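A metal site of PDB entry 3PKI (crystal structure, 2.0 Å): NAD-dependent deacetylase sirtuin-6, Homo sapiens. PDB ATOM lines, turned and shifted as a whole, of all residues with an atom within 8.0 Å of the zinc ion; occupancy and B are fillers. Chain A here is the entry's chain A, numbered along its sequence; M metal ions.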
ATOM      1  N   GLU A 140     -11.040  20.501 -20.569  1.00  0.00           N
ATOM      2  CA  GLU A 140     -10.413  21.810 -20.655  1.00  0.00           C
ATOM      3  C   GLU A 140     -11.033  22.671 -21.757  1.00  0.00           C
ATOM      4  O   GLU A 140     -11.327  22.150 -22.837  1.00  0.00           O
ATOM      5  CB  GLU A 140      -8.911  21.598 -20.930  1.00  0.00           C
ATOM      6  CG  GLU A 140      -8.050  22.851 -20.837  1.00  0.00           C
ATOM      7  CD  GLU A 140      -6.569  22.553 -20.971  1.00  0.00           C
ATOM      8  OE1 GLU A 140      -5.933  23.105 -21.887  1.00  0.00           O
ATOM      9  OE2 GLU A 140      -6.054  21.740 -20.168  1.00  0.00           O
ATOM     10  N   CYS A 141     -11.236  23.981 -21.478  1.00  0.00           N
ATOM     11  CA  CYS A 141     -11.779  24.930 -22.472  1.00  0.00           C
ATOM     12  C   CYS A 141     -10.745  25.141 -23.550  1.00  0.00           C
ATOM     13  O   CYS A 141      -9.600  25.472 -23.248  1.00  0.00           O
ATOM     14  CB  CYS A 141     -12.199  26.247 -21.828  1.00  0.00           C
ATOM     15  SG  CYS A 141     -12.719  27.516 -23.027  1.00  0.00           S
ATOM     16  N   ALA A 142     -11.145  24.948 -24.825  1.00  0.00           N
ATOM     17  CA  ALA A 142     -10.258  25.127 -25.984  1.00  0.00           C
ATOM     18  C   ALA A 142      -9.740  26.579 -26.126  1.00  0.00           C
ATOM     19  O   ALA A 142      -8.680  26.781 -26.709  1.00  0.00           O
ATOM     20  CB  ALA A 142     -10.974  24.683 -27.264  1.00  0.00           C
ATOM     21  N   LYS A 143     -10.484  27.576 -25.553  1.00  0.00           N
ATOM     22  CA  LYS A 143     -10.126  29.000 -25.610  1.00  0.00           C
ATOM     23  C   LYS A 143      -9.290  29.471 -24.398  1.00  0.00           C
ATOM     24  O   LYS A 143      -8.085  29.692 -24.553  1.00  0.00           O
ATOM     25  CB  LYS A 143     -11.380  29.887 -25.771  1.00  0.00           C
ATOM     26  CG  LYS A 143     -12.098  29.729 -27.112  1.00  0.00           C
ATOM     27  CD  LYS A 143     -12.895  30.982 -27.452  1.00  0.00           C
ATOM     28  CE  LYS A 143     -12.284  31.779 -28.593  1.00  0.00           C
ATOM     29  NZ  LYS A 143     -10.957  32.360 -28.230  1.00  0.00           N
ATOM     30  N   CYS A 144      -9.910  29.635 -23.205  1.00  0.00           N
ATOM     31  CA  CYS A 144      -9.253  30.179 -21.989  1.00  0.00           C
ATOM     32  C   CYS A 144      -8.362  29.181 -21.212  1.00  0.00           C
ATOM     33  O   CYS A 144      -7.652  29.608 -20.291  1.00  0.00           O
ATOM     34  CB  CYS A 144     -10.298  30.805 -21.071  1.00  0.00           C
ATOM     35  SG  CYS A 144     -11.481  29.627 -20.367  1.00  0.00           S
ATOM     36  N   LYS A 145      -8.410  27.869 -21.560  1.00  0.00           N
ATOM     37  CA  LYS A 145      -7.622  26.780 -20.932  1.00  0.00           C
ATOM     38  C   LYS A 145      -8.126  26.412 -19.506  1.00  0.00           C
ATOM     39  O   LYS A 145      -7.433  25.664 -18.804  1.00  0.00           O
ATOM     40  CB  LYS A 145      -6.089  27.060 -20.917  1.00  0.00           C
ATOM     41  CG  LYS A 145      -5.397  27.392 -22.257  1.00  0.00           C
ATOM     42  CD  LYS A 145      -5.981  26.660 -23.463  1.00  0.00           C
ATOM     43  CE  LYS A 145      -5.126  26.731 -24.689  1.00  0.00           C
ATOM     44  NZ  LYS A 145      -5.845  26.215 -25.881  1.00  0.00           N
ATOM     45  N   THR A 146      -9.311  26.918 -19.093  1.00  0.00           N
ATOM     46  CA  THR A 146      -9.888  26.607 -17.777  1.00  0.00           C
ATOM     47  C   THR A 146     -10.201  25.095 -17.742  1.00  0.00           C
ATOM     48  O   THR A 146     -10.753  24.553 -18.692  1.00  0.00           O
ATOM     49  CB  THR A 146     -11.098  27.506 -17.446  1.00  0.00           C
ATOM     50  OG1 THR A 146     -10.645  28.857 -17.382  1.00  0.00           O
ATOM     51  CG2 THR A 146     -11.768  27.146 -16.112  1.00  0.00           C
ATOM     52  N   GLN A 147      -9.779  24.440 -16.657  1.00  0.00           N
ATOM     53  CA  GLN A 147      -9.993  23.004 -16.478  1.00  0.00           C
ATOM     54  C   GLN A 147     -11.163  22.757 -15.537  1.00  0.00           C
ATOM     55  O   GLN A 147     -11.394  23.531 -14.610  1.00  0.00           O
ATOM     56  CB  GLN A 147      -8.716  22.323 -15.970  1.00  0.00           C
ATOM     57  CG  GLN A 147      -7.555  22.409 -16.968  1.00  0.00           C
ATOM     58  CD  GLN A 147      -6.341  21.613 -16.555  1.00  0.00           C
ATOM     59  OE1 GLN A 147      -6.047  21.442 -15.365  1.00  0.00           O
ATOM     60  NE2 GLN A 147      -5.579  21.153 -17.527  1.00  0.00           N
ATOM     61  N   TYR A 148     -11.932  21.704 -15.835  1.00  0.00           N
ATOM     62  CA  TYR A 148     -13.101  21.312 -15.066  1.00  0.00           C
ATOM     63  C   TYR A 148     -12.898  19.894 -14.552  1.00  0.00           C
ATOM     64  O   TYR A 148     -12.826  18.960 -15.357  1.00  0.00           O
ATOM     65  CB  TYR A 148     -14.391  21.397 -15.944  1.00  0.00           C
ATOM     66  CG  TYR A 148     -14.732  22.808 -16.361  1.00  0.00           C
ATOM     67  CD1 TYR A 148     -14.076  23.415 -17.425  1.00  0.00           C
ATOM     68  CD2 TYR A 148     -15.685  23.546 -15.668  1.00  0.00           C
ATOM     69  CE1 TYR A 148     -14.345  24.731 -17.787  1.00  0.00           C
ATOM     70  CE2 TYR A 148     -15.976  24.862 -16.030  1.00  0.00           C
ATOM     71  CZ  TYR A 148     -15.311  25.451 -17.103  1.00  0.00           C
ATOM     72  OH  TYR A 148     -15.602  26.738 -17.472  1.00  0.00           O
ATOM     73  N   LEU A 165     -19.966  23.408 -22.795  1.00  0.00           N
ATOM     74  CA  LEU A 165     -19.357  24.718 -23.002  1.00  0.00           C
ATOM     75  C   LEU A 165     -18.740  25.258 -21.740  1.00  0.00           C
ATOM     76  O   LEU A 165     -19.201  24.915 -20.631  1.00  0.00           O
ATOM     77  CB  LEU A 165     -20.399  25.731 -23.528  1.00  0.00           C
ATOM     78  CG  LEU A 165     -21.072  25.432 -24.881  1.00  0.00           C
ATOM     79  CD1 LEU A 165     -22.126  26.487 -25.186  1.00  0.00           C
ATOM     80  CD2 LEU A 165     -20.049  25.354 -26.026  1.00  0.00           C
ATOM     81  N   CYS A 166     -17.740  26.138 -21.889  1.00  0.00           N
ATOM     82  CA  CYS A 166     -17.076  26.825 -20.766  1.00  0.00           C
ATOM     83  C   CYS A 166     -18.118  27.688 -20.051  1.00  0.00           C
ATOM     84  O   CYS A 166     -19.046  28.184 -20.709  1.00  0.00           O
ATOM     85  CB  CYS A 166     -15.912  27.670 -21.267  1.00  0.00           C
ATOM     86  SG  CYS A 166     -14.906  28.382 -19.955  1.00  0.00           S
ATOM     87  N   THR A 167     -18.000  27.833 -18.737  1.00  0.00           N
ATOM     88  CA  THR A 167     -18.997  28.609 -17.989  1.00  0.00           C
ATOM     89  C   THR A 167     -18.346  29.745 -17.183  1.00  0.00           C
ATOM     90  O   THR A 167     -19.020  30.299 -16.304  1.00  0.00           O
ATOM     91  CB  THR A 167     -19.890  27.675 -17.128  1.00  0.00           C
ATOM     92  OG1 THR A 167     -19.084  26.779 -16.379  1.00  0.00           O
ATOM     93  CG2 THR A 167     -20.897  26.880 -17.963  1.00  0.00           C
ATOM     94  N   VAL A 168     -17.080  30.135 -17.499  1.00  0.00           N
ATOM     95  CA  VAL A 168     -16.416  31.243 -16.788  1.00  0.00           C
ATOM     96  C   VAL A 168     -17.141  32.570 -17.162  1.00  0.00           C
ATOM     97  O   VAL A 168     -17.244  32.918 -18.344  1.00  0.00           O
ATOM     98  CB  VAL A 168     -14.856  31.325 -16.919  1.00  0.00           C
ATOM     99  CG1 VAL A 168     -14.193  30.062 -16.382  1.00  0.00           C
ATOM    100  CG2 VAL A 168     -14.401  31.615 -18.334  1.00  0.00           C
ATOM    101  N   ALA A 176     -18.000  36.711 -20.743  1.00  0.00           N
ATOM    102  CA  ALA A 176     -18.211  35.257 -20.643  1.00  0.00           C
ATOM    103  C   ALA A 176     -17.489  34.528 -21.794  1.00  0.00           C
ATOM    104  O   ALA A 176     -17.337  35.102 -22.882  1.00  0.00           O
ATOM    105  CB  ALA A 176     -19.703  34.940 -20.676  1.00  0.00           C
ATOM    106  N   CYS A 177     -17.015  33.302 -21.533  1.00  0.00           N
ATOM    107  CA  CYS A 177     -16.229  32.560 -22.527  1.00  0.00           C
ATOM    108  C   CYS A 177     -17.081  31.813 -23.558  1.00  0.00           C
ATOM    109  O   CYS A 177     -16.924  32.064 -24.761  1.00  0.00           O
ATOM    110  CB  CYS A 177     -15.254  31.625 -21.837  1.00  0.00           C
ATOM    111  SG  CYS A 177     -14.102  30.806 -22.964  1.00  0.00           S
ATOM    112  N   ARG A 178     -17.922  30.843 -23.103  1.00  0.00           N
ATOM    113  CA  ARG A 178     -18.767  29.966 -23.918  1.00  0.00           C
ATOM    114  C   ARG A 178     -17.922  29.056 -24.857  1.00  0.00           C
ATOM    115  O   ARG A 178     -18.452  28.460 -25.798  1.00  0.00           O
ATOM    116  CB  ARG A 178     -19.836  30.755 -24.713  1.00  0.00           C
ATOM    117  N   GLY A 179     -16.622  28.927 -24.552  1.00  0.00           N
ATOM    118  CA  GLY A 179     -15.669  28.097 -25.290  1.00  0.00           C
ATOM    119  C   GLY A 179     -16.000  26.618 -25.260  1.00  0.00           C
ATOM    120  O   GLY A 179     -16.735  26.150 -24.380  1.00  0.00           O
ATOM    121  N   GLU A 180     -15.479  25.874 -26.236  1.00  0.00           N
ATOM    122  CA  GLU A 180     -15.708  24.436 -26.377  1.00  0.00           C
ATOM    123  C   GLU A 180     -14.857  23.652 -25.378  1.00  0.00           C
ATOM    124  O   GLU A 180     -13.646  23.833 -25.327  1.00  0.00           O
ATOM    125  CB  GLU A 180     -15.383  24.023 -27.821  1.00  0.00           C
ATOM    126  CG  GLU A 180     -15.811  22.625 -28.217  1.00  0.00           C
ATOM    127  CD  GLU A 180     -15.496  22.312 -29.656  1.00  0.00           C
ATOM    128  OE1 GLU A 180     -14.328  21.990 -29.962  1.00  0.00           O
ATOM    129  OE2 GLU A 180     -16.418  22.406 -30.508  1.00  0.00           O
ATOM    130  N   LEU A 181     -15.505  22.794 -24.570  1.00  0.00           N
ATOM    131  CA  LEU A 181     -14.796  21.944 -23.613  1.00  0.00           C
ATOM    132  C   LEU A 181     -14.355  20.679 -24.321  1.00  0.00           C
ATOM    133  O   LEU A 181     -15.138  20.078 -25.072  1.00  0.00           O
ATOM    134  CB  LEU A 181     -15.646  21.602 -22.373  1.00  0.00           C
ATOM    135  CG  LEU A 181     -16.139  22.758 -21.487  1.00  0.00           C
ATOM    136  CD1 LEU A 181     -16.786  22.227 -20.225  1.00  0.00           C
ATOM    137  CD2 LEU A 181     -15.016  23.707 -21.134  1.00  0.00           C
HETATM  138 ZN    ZN M   1     -13.291  29.043 -21.412  1.00  0.00          ZN
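The side-chain sulfur (SG) of Cys 141 sits close to the backbone NH (N) of Lys 143 (3.4 Å). The side-chain sulfur (SG) of Cys 166 lies close to the side-chain hydroxyl (OH) of Tyr 148, at 3.1 Å. The backbone carbonyl oxygen of Thr 146 is in hydrogen-bond range of the backbone NH of Cys 141 (2.9 Å). O of Gly 179 sits at hydrogen-bond distance from N of Cys 166 (2.7 Å). The side-chain sulfur (SG) of Cys 166 sits close to the backbone NH (N) of Val 168. The side-chain hydroxyl (OG1) of Thr 146 lies close to the side-chain sulfur (SG) of Cys 144 (3.2 Å). The backbone NH (N) of Cys 177 lies within hydrogen-bond range of the backbone carbonyl oxygen (O) of Val 168, at 3.2 Å. The side-chain sulfur of Cys 177 sits close to the backbone NH of Gly 179 (3.5 Å).
Within 4 Å of the zinc ion: Cys 141, Cys 144, Cys 166 and Cys 177.
The zinc ion is bound by SG of Cys 144 (2.2 Å), SG of Cys 166 (2.3 Å), SG of Cys 141 (2.3 Å) and SG of Cys 177 (2.5 Å). The zinc ion has four donor atoms within binding distance.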
